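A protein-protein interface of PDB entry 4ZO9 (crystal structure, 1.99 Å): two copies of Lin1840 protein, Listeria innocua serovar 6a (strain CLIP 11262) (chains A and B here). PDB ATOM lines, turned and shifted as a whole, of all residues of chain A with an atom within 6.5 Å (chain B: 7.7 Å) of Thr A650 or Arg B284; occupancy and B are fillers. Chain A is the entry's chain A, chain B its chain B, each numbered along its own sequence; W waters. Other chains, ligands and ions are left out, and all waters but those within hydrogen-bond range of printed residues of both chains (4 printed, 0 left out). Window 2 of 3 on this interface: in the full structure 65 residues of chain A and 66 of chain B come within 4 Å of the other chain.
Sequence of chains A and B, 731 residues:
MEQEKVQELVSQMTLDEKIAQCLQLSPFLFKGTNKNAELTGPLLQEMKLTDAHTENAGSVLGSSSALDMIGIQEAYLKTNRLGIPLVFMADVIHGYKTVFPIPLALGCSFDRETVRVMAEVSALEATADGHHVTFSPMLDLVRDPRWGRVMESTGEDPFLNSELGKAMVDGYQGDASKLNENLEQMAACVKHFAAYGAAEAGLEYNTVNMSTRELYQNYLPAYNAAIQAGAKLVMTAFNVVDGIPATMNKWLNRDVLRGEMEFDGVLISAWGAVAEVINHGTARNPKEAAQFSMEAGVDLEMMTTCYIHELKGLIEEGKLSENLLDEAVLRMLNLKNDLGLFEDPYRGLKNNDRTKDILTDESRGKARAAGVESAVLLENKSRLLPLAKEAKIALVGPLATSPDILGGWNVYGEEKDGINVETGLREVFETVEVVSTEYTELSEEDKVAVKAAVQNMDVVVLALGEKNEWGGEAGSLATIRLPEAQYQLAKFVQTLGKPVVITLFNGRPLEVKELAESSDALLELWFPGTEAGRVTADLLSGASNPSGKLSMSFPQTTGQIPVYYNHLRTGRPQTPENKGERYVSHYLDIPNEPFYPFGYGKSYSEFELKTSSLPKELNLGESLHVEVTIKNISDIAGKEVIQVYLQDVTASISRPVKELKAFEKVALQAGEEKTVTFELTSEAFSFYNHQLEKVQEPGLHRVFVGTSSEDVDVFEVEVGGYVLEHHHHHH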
ATOM      1  N   ASP A 648     -24.869   8.630  24.987  1.00  0.00           N
ATOM      2  CA  ASP A 648     -24.271   7.313  24.990  1.00  0.00           C
ATOM      3  C   ASP A 648     -23.516   7.099  23.691  1.00  0.00           C
ATOM      4  O   ASP A 648     -24.102   6.843  22.655  1.00  0.00           O
ATOM      5  CB  ASP A 648     -25.376   6.282  25.155  1.00  0.00           C
ATOM      6  CG  ASP A 648     -24.876   4.911  25.462  1.00  0.00           C
ATOM      7  OD1 ASP A 648     -23.626   4.573  25.318  1.00  0.00           O
ATOM      8  OD2 ASP A 648     -25.771   4.147  25.830  1.00  0.00           O
ATOM      9  N   VAL A 649     -22.195   7.124  23.751  1.00  0.00           N
ATOM     10  CA  VAL A 649     -21.368   7.217  22.534  1.00  0.00           C
ATOM     11  C   VAL A 649     -21.506   6.001  21.619  1.00  0.00           C
ATOM     12  O   VAL A 649     -21.601   6.148  20.391  1.00  0.00           O
ATOM     13  CB  VAL A 649     -19.906   7.525  22.907  1.00  0.00           C
ATOM     14  CG1 VAL A 649     -19.015   7.541  21.711  1.00  0.00           C
ATOM     15  CG2 VAL A 649     -19.854   8.902  23.609  1.00  0.00           C
ATOM     16  N   THR A 650     -21.553   4.817  22.230  1.00  0.00           N
ATOM     17  CA  THR A 650     -21.616   3.557  21.532  1.00  0.00           C
ATOM     18  C   THR A 650     -22.532   2.690  22.265  1.00  0.00           C
ATOM     19  O   THR A 650     -22.402   2.546  23.481  1.00  0.00           O
ATOM     20  CB  THR A 650     -20.251   2.855  21.559  1.00  0.00           C
ATOM     21  OG1 THR A 650     -19.235   3.834  21.256  1.00  0.00           O
ATOM     22  CG2 THR A 650     -20.220   1.737  20.582  1.00  0.00           C
ATOM     23  N   ALA A 651     -23.473   2.102  21.555  1.00  0.00           N
ATOM     24  CA  ALA A 651     -24.529   1.346  22.208  1.00  0.00           C
ATOM     25  C   ALA A 651     -25.062   0.310  21.225  1.00  0.00           C
ATOM     26  O   ALA A 651     -24.744   0.376  20.076  1.00  0.00           O
ATOM     27  CB  ALA A 651     -25.631   2.307  22.699  1.00  0.00           C
ATOM     28  N   SER A 652     -25.828  -0.667  21.704  1.00  0.00           N
ATOM     29  CA  SER A 652     -26.408  -1.701  20.824  1.00  0.00           C
ATOM     30  C   SER A 652     -27.589  -1.173  19.975  1.00  0.00           C
ATOM     31  O   SER A 652     -28.086  -1.860  19.114  1.00  0.00           O
ATOM     32  CB  SER A 652     -26.881  -2.914  21.633  1.00  0.00           C
ATOM     33  OG  SER A 652     -27.859  -2.517  22.581  1.00  0.00           O
ATOM     34  N   ILE A 653     -28.035   0.034  20.280  1.00  0.00           N
ATOM     35  CA  ILE A 653     -28.974   0.825  19.474  1.00  0.00           C
ATOM     36  C   ILE A 653     -28.272   2.182  19.265  1.00  0.00           C
ATOM     37  O   ILE A 653     -27.577   2.663  20.180  1.00  0.00           O
ATOM     38  CB  ILE A 653     -30.261   1.098  20.298  1.00  0.00           C
ATOM     39  CG1 ILE A 653     -30.997  -0.196  20.570  1.00  0.00           C
ATOM     40  CG2 ILE A 653     -31.137   2.126  19.617  1.00  0.00           C
ATOM     41  CD1 ILE A 653     -31.472  -0.925  19.323  1.00  0.00           C
ATOM     42  N   ARG A 655     -27.915   5.732  19.494  1.00  0.00           N
ATOM     43  CA  ARG A 655     -28.479   6.590  20.529  1.00  0.00           C
ATOM     44  C   ARG A 655     -28.400   8.050  20.139  1.00  0.00           C
ATOM     45  O   ARG A 655     -27.570   8.444  19.334  1.00  0.00           O
ATOM     46  CB  ARG A 655     -27.787   6.339  21.907  1.00  0.00           C
ATOM     47  CG  ARG A 655     -28.020   4.924  22.460  1.00  0.00           C
ATOM     48  CD  ARG A 655     -29.290   4.729  23.285  1.00  0.00           C
ATOM     49  NE  ARG A 655     -29.245   5.562  24.445  1.00  0.00           N
ATOM     50  CZ  ARG A 655     -30.194   6.413  24.858  1.00  0.00           C
ATOM     51  NH1 ARG A 655     -31.342   6.601  24.219  1.00  0.00           N
ATOM     52  NH2 ARG A 655     -29.962   7.137  25.921  1.00  0.00           N
ATOM     53  N   GLU A 697     -25.798  -0.402  29.687  1.00  0.00           N
ATOM     54  CA  GLU A 697     -24.620  -0.964  29.082  1.00  0.00           C
ATOM     55  C   GLU A 697     -23.368  -0.215  29.578  1.00  0.00           C
ATOM     56  O   GLU A 697     -23.324   1.027  29.560  1.00  0.00           O
ATOM     57  CB  GLU A 697     -24.718  -0.832  27.552  1.00  0.00           C
ATOM     58  CG  GLU A 697     -25.618  -1.880  26.932  1.00  0.00           C
ATOM     59  CD  GLU A 697     -25.904  -1.640  25.459  1.00  0.00           C
ATOM     60  OE1 GLU A 697     -25.378  -0.659  24.894  1.00  0.00           O
ATOM     61  OE2 GLU A 697     -26.663  -2.455  24.886  1.00  0.00           O
ATOM     62  N   PRO A 698     -22.320  -0.961  29.973  1.00  0.00           N
ATOM     63  CA  PRO A 698     -21.020  -0.285  30.200  1.00  0.00           C
ATOM     64  C   PRO A 698     -20.443   0.421  28.967  1.00  0.00           C
ATOM     65  O   PRO A 698     -20.744   0.055  27.815  1.00  0.00           O
ATOM     66  CB  PRO A 698     -20.079  -1.406  30.610  1.00  0.00           C
ATOM     67  CG  PRO A 698     -20.695  -2.653  30.093  1.00  0.00           C
ATOM     68  CD  PRO A 698     -22.201  -2.426  30.101  1.00  0.00           C
ATOM     69  N   GLY A 699     -19.618   1.434  29.241  1.00  0.00           N
ATOM     70  CA  GLY A 699     -19.015   2.209  28.203  1.00  0.00           C
ATOM     71  C   GLY A 699     -19.060   3.691  28.445  1.00  0.00           C
ATOM     72  O   GLY A 699     -19.393   4.146  29.547  1.00  0.00           O
ATOM     73  N   LEU A 700     -18.748   4.450  27.378  1.00  0.00           N
ATOM     74  CA  LEU A 700     -18.493   5.868  27.472  1.00  0.00           C
ATOM     75  C   LEU A 700     -19.756   6.711  27.309  1.00  0.00           C
ATOM     76  O   LEU A 700     -20.559   6.438  26.432  1.00  0.00           O
ATOM     77  CB  LEU A 700     -17.482   6.278  26.398  1.00  0.00           C
ATOM     78  CG  LEU A 700     -17.009   7.743  26.389  1.00  0.00           C
ATOM     79  CD1 LEU A 700     -16.212   8.069  27.639  1.00  0.00           C
ATOM     80  CD2 LEU A 700     -16.214   8.037  25.107  1.00  0.00           C
ATOM     81  N   HIS A 701     -19.894   7.731  28.140  1.00  0.00           N
ATOM     82  CA  HIS A 701     -20.961   8.712  28.023  1.00  0.00           C
ATOM     83  C   HIS A 701     -20.312  10.064  28.063  1.00  0.00           C
ATOM     84  O   HIS A 701     -19.224  10.267  28.714  1.00  0.00           O
ATOM     85  CB  HIS A 701     -21.947   8.596  29.161  1.00  0.00           C
ATOM     86  CG  HIS A 701     -22.745   7.315  29.147  1.00  0.00           C
ATOM     87  ND1 HIS A 701     -24.052   7.258  28.737  1.00  0.00           N
ATOM     88  CD2 HIS A 701     -22.401   6.041  29.466  1.00  0.00           C
ATOM     89  CE1 HIS A 701     -24.477   6.003  28.783  1.00  0.00           C
ATOM     90  NE2 HIS A 701     -23.496   5.246  29.239  1.00  0.00           N
ATOM     91  N   GLU A 718     -16.593   7.293  31.849  1.00  0.00           N
ATOM     92  CA  GLU A 718     -16.577   5.894  31.463  1.00  0.00           C
ATOM     93  C   GLU A 718     -17.317   5.050  32.510  1.00  0.00           C
ATOM     94  O   GLU A 718     -16.858   4.951  33.674  1.00  0.00           O
ATOM     95  CB  GLU A 718     -15.126   5.448  31.367  1.00  0.00           C
ATOM     96  CG  GLU A 718     -14.949   4.115  30.695  1.00  0.00           C
ATOM     97  CD  GLU A 718     -15.359   4.130  29.236  1.00  0.00           C
ATOM     98  OE1 GLU A 718     -16.002   3.135  28.855  1.00  0.00           O
ATOM     99  OE2 GLU A 718     -15.044   5.088  28.490  1.00  0.00           O
ATOM    100  N   VAL B 277     -20.706   2.090  10.713  1.00  0.00           N
ATOM    101  CA  VAL B 277     -21.476   1.733  11.888  1.00  0.00           C
ATOM    102  C   VAL B 277     -20.823   2.381  13.138  1.00  0.00           C
ATOM    103  O   VAL B 277     -21.516   2.579  14.161  1.00  0.00           O
ATOM    104  CB  VAL B 277     -21.680   0.221  12.094  1.00  0.00           C
ATOM    105  CG1 VAL B 277     -22.245  -0.439  10.841  1.00  0.00           C
ATOM    106  CG2 VAL B 277     -20.391  -0.430  12.570  1.00  0.00           C
ATOM    107  N   ILE B 278     -19.528   2.747  13.021  1.00  0.00           N
ATOM    108  CA  ILE B 278     -18.865   3.478  14.088  1.00  0.00           C
ATOM    109  C   ILE B 278     -19.519   4.853  14.200  1.00  0.00           C
ATOM    110  O   ILE B 278     -19.942   5.252  15.273  1.00  0.00           O
ATOM    111  CB  ILE B 278     -17.353   3.565  13.924  1.00  0.00           C
ATOM    112  CG1 ILE B 278     -16.775   2.165  13.941  1.00  0.00           C
ATOM    113  CG2 ILE B 278     -16.744   4.461  15.004  1.00  0.00           C
ATOM    114  CD1 ILE B 278     -15.519   1.962  13.111  1.00  0.00           C
ATOM    115  N   ASN B 279     -19.680   5.536  13.097  1.00  0.00           N
ATOM    116  CA  ASN B 279     -20.298   6.849  13.104  1.00  0.00           C
ATOM    117  C   ASN B 279     -21.690   6.807  13.660  1.00  0.00           C
ATOM    118  O   ASN B 279     -22.070   7.699  14.378  1.00  0.00           O
ATOM    119  CB  ASN B 279     -20.325   7.486  11.702  1.00  0.00           C
ATOM    120  CG  ASN B 279     -18.947   7.826  11.185  1.00  0.00           C
ATOM    121  OD1 ASN B 279     -18.060   8.103  11.950  1.00  0.00           O
ATOM    122  ND2 ASN B 279     -18.774   7.824   9.881  1.00  0.00           N
ATOM    123  N   HIS B 280     -22.431   5.750  13.346  1.00  0.00           N
ATOM    124  CA  HIS B 280     -23.779   5.540  13.871  1.00  0.00           C
ATOM    125  C   HIS B 280     -23.790   5.313  15.379  1.00  0.00           C
ATOM    126  O   HIS B 280     -24.843   5.409  16.012  1.00  0.00           O
ATOM    127  CB  HIS B 280     -24.408   4.291  13.257  1.00  0.00           C
ATOM    128  CG  HIS B 280     -25.120   4.484  11.944  1.00  0.00           C
ATOM    129  ND1 HIS B 280     -26.366   5.077  11.836  1.00  0.00           N
ATOM    130  CD2 HIS B 280     -24.811   4.034  10.711  1.00  0.00           C
ATOM    131  CE1 HIS B 280     -26.783   5.000  10.589  1.00  0.00           C
ATOM    132  NE2 HIS B 280     -25.847   4.387   9.877  1.00  0.00           N
ATOM    133  N   GLY B 281     -22.657   5.002  15.970  1.00  0.00           N
ATOM    134  CA  GLY B 281     -22.621   4.725  17.410  1.00  0.00           C
ATOM    135  C   GLY B 281     -22.998   3.316  17.888  1.00  0.00           C
ATOM    136  O   GLY B 281     -23.396   3.160  19.002  1.00  0.00           O
ATOM    137  N   THR B 282     -22.860   2.303  17.044  1.00  0.00           N
ATOM    138  CA  THR B 282     -23.120   0.917  17.373  1.00  0.00           C
ATOM    139  C   THR B 282     -21.904  -0.008  17.213  1.00  0.00           C
ATOM    140  O   THR B 282     -21.979  -1.265  17.239  1.00  0.00           O
ATOM    141  CB  THR B 282     -24.317   0.392  16.578  1.00  0.00           C
ATOM    142  OG1 THR B 282     -24.045   0.490  15.187  1.00  0.00           O
ATOM    143  CG2 THR B 282     -25.617   1.186  16.932  1.00  0.00           C
ATOM    144  N   ALA B 283     -20.768   0.624  17.090  1.00  0.00           N
ATOM    145  CA  ALA B 283     -19.456  -0.065  17.164  1.00  0.00           C
ATOM    146  C   ALA B 283     -18.524   1.007  17.674  1.00  0.00           C
ATOM    147  O   ALA B 283     -18.708   2.184  17.315  1.00  0.00           O
ATOM    148  CB  ALA B 283     -19.032  -0.545  15.822  1.00  0.00           C
ATOM    149  N   ARG B 284     -17.609   0.624  18.561  1.00  0.00           N
ATOM    150  CA  ARG B 284     -16.627   1.578  19.116  1.00  0.00           C
ATOM    151  C   ARG B 284     -15.481   1.874  18.163  1.00  0.00           C
ATOM    152  O   ARG B 284     -14.872   2.888  18.241  1.00  0.00           O
ATOM    153  CB  ARG B 284     -16.075   1.084  20.505  1.00  0.00           C
ATOM    154  CG  ARG B 284     -15.332   2.159  21.285  1.00  0.00           C
ATOM    155  CD  ARG B 284     -14.523   1.583  22.454  1.00  0.00           C
ATOM    156  NE  ARG B 284     -15.213   1.664  23.717  1.00  0.00           N
ATOM    157  CZ  ARG B 284     -14.906   2.474  24.747  1.00  0.00           C
ATOM    158  NH1 ARG B 284     -13.899   3.344  24.684  1.00  0.00           N
ATOM    159  NH2 ARG B 284     -15.623   2.427  25.881  1.00  0.00           N
ATOM    160  N   ASN B 285     -15.206   0.976  17.255  1.00  0.00           N
ATOM    161  CA  ASN B 285     -13.913   0.954  16.577  1.00  0.00           C
ATOM    162  C   ASN B 285     -13.925  -0.041  15.447  1.00  0.00           C
ATOM    163  O   ASN B 285     -14.875  -0.830  15.345  1.00  0.00           O
ATOM    164  CB  ASN B 285     -12.734   0.687  17.519  1.00  0.00           C
ATOM    165  CG  ASN B 285     -12.817  -0.630  18.269  1.00  0.00           C
ATOM    166  OD1 ASN B 285     -13.348  -1.627  17.807  1.00  0.00           O
ATOM    167  ND2 ASN B 285     -12.225  -0.645  19.431  1.00  0.00           N
ATOM    168  N   PRO B 286     -12.898  -0.005  14.571  1.00  0.00           N
ATOM    169  CA  PRO B 286     -12.988  -0.960  13.414  1.00  0.00           C
ATOM    170  C   PRO B 286     -12.932  -2.450  13.759  1.00  0.00           C
ATOM    171  O   PRO B 286     -13.380  -3.309  12.970  1.00  0.00           O
ATOM    172  CB  PRO B 286     -11.838  -0.535  12.509  1.00  0.00           C
ATOM    173  CG  PRO B 286     -11.589   0.908  12.875  1.00  0.00           C
ATOM    174  CD  PRO B 286     -11.928   1.086  14.338  1.00  0.00           C
ATOM    175  N   LYS B 287     -12.421  -2.780  14.935  1.00  0.00           N
ATOM    176  CA  LYS B 287     -12.463  -4.196  15.389  1.00  0.00           C
ATOM    177  C   LYS B 287     -13.923  -4.627  15.694  1.00  0.00           C
ATOM    178  O   LYS B 287     -14.381  -5.692  15.293  1.00  0.00           O
ATOM    179  CB  LYS B 287     -11.549  -4.381  16.625  1.00  0.00           C
ATOM    180  CG  LYS B 287     -11.515  -5.784  17.192  1.00  0.00           C
ATOM    181  CD  LYS B 287     -10.772  -5.806  18.531  1.00  0.00           C
ATOM    182  CE  LYS B 287     -10.084  -7.165  18.728  1.00  0.00           C
ATOM    183  NZ  LYS B 287      -8.884  -7.067  19.600  1.00  0.00           N
ATOM    184  N   GLU B 288     -14.661  -3.776  16.374  1.00  0.00           N
ATOM    185  CA  GLU B 288     -16.085  -4.043  16.660  1.00  0.00           C
ATOM    186  C   GLU B 288     -16.952  -4.039  15.382  1.00  0.00           C
ATOM    187  O   GLU B 288     -17.812  -4.896  15.218  1.00  0.00           O
ATOM    188  CB  GLU B 288     -16.640  -3.044  17.696  1.00  0.00           C
ATOM    189  CG  GLU B 288     -16.237  -3.392  19.120  1.00  0.00           C
ATOM    190  CD  GLU B 288     -16.953  -2.645  20.196  1.00  0.00           C
ATOM    191  OE1 GLU B 288     -17.903  -1.875  19.875  1.00  0.00           O
ATOM    192  OE2 GLU B 288     -16.546  -2.842  21.382  1.00  0.00           O
ATOM    193  N   ALA B 289     -16.685  -3.094  14.473  1.00  0.00           N
ATOM    194  CA  ALA B 289     -17.345  -3.023  13.179  1.00  0.00           C
ATOM    195  C   ALA B 289     -17.202  -4.271  12.347  1.00  0.00           C
ATOM    196  O   ALA B 289     -18.217  -4.825  11.837  1.00  0.00           O
ATOM    197  CB  ALA B 289     -16.832  -1.832  12.412  1.00  0.00           C
ATOM    198  N   PHE B 292     -18.972  -7.289  14.086  1.00  0.00           N
ATOM    199  CA  PHE B 292     -20.452  -7.233  14.012  1.00  0.00           C
ATOM    200  C   PHE B 292     -20.934  -7.427  12.573  1.00  0.00           C
ATOM    201  O   PHE B 292     -21.914  -8.102  12.320  1.00  0.00           O
ATOM    202  CB  PHE B 292     -21.006  -5.931  14.631  1.00  0.00           C
ATOM    203  CG  PHE B 292     -20.608  -5.723  16.060  1.00  0.00           C
ATOM    204  CD1 PHE B 292     -20.414  -6.804  16.920  1.00  0.00           C
ATOM    205  CD2 PHE B 292     -20.529  -4.436  16.586  1.00  0.00           C
ATOM    206  CE1 PHE B 292     -20.093  -6.595  18.253  1.00  0.00           C
ATOM    207  CE2 PHE B 292     -20.177  -4.228  17.923  1.00  0.00           C
ATOM    208  CZ  PHE B 292     -19.957  -5.313  18.751  1.00  0.00           C
HETATM  209  O   HOH W   1     -18.554   3.369  24.927  1.00  0.00           O
HETATM  210  O   HOH W   2     -24.986   5.176  20.178  1.00  0.00           O
HETATM  211  O   HOH W   3     -19.026   4.521  18.408  1.00  0.00           O
HETATM  212  O   HOH W   4     -26.825   8.123  16.844  1.00  0.00           O
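Asp A648 touches none of the printed residues of chain B.
Of chain B, only Gly B281 (3.1 Å), Ala B283 (3.4 Å) and Arg B284 (3.5 Å) come within 4 Å of Thr A650.
Of the printed residues of chain B, Ile A653 touches Thr B282 (3.7 Å).
His A701 touches none of the printed residues of chain B.
Of the printed residues of chain A, Ala B283 touches Thr A650 (3.4 Å).
Of the printed residues of chain A, Arg B284 touches Thr A650 and Glu A718.
The nearest printed residue of chain A that does not touch Arg B284 is Leu A700 (4.01 Å).
Gly B281 touches Val A649.
Thr A650 touches Gly B281.
CG2 of Thr A650 touches C of Ala B283, at 3.4 Å.
Thr A650 touches Arg B284.
O of Ala A651 touches CA of Thr B282, at 3.2 Å.
Thr B282 touches Ile A653 (CG2 to C, 3.7 Å).
The side-chain carboxylate (OE1) of Glu A718 lies within salt-bridge range of the guanidinium group (NH2) of Arg B284.
N of Ala A651 is in hydrogen-bond range of O of Gly B281 (2.8 Å).
The backbone NH (N) of Leu A700 sits at hydrogen-bond distance from the side-chain carboxylate (OE1) of Glu A718, at 3.4 Å.
The backbone carbonyl oxygen (O) of Leu A700 lies within hydrogen-bond range of the backbone NH (N) of Val A649, 3.2 Å away.
The backbone carbonyl oxygen (O) of Val B277 is in hydrogen-bond range of the backbone NH (N) of Thr B282, 3.2 Å away.
N of Arg B284 sits at hydrogen-bond distance from OE1 of Glu B288 (2.8 Å).
Water W3 lies within hydrogen-bond range of the backbone carbonyl oxygen (O) of Ala B283 (2.6 Å), the side-chain hydroxyl (OG1) of Thr A650 (2.9 Å) and the backbone carbonyl oxygen (O) of Ile B278 (3.3 Å).
Water W4 bridges O of Arg A655 and O of His B280.
Water W1 bridges the backbone NH of Leu A700 and the guanidinium group of Arg B284.
Water W2 lies within hydrogen-bond range of O of Gly B281, N of Arg A655 and O of Asp A648.
No position is printed for both chains.
Of the 13 printed residues of chain A, 5 touch a printed residue of chain B.
Printed residues of chain A that touch a printed residue of chain B: Val A649, Thr A650, Ala A651, Ile A653 and Glu A718.
Among the printed residues, 8 pairs touch across the chains.
Among the printed residues, Asp or Glu carboxylates within 4 Å of a Lys or Arg side-chain nitrogen of the other chain: Glu A718 with Arg B284 (3.1 Å).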
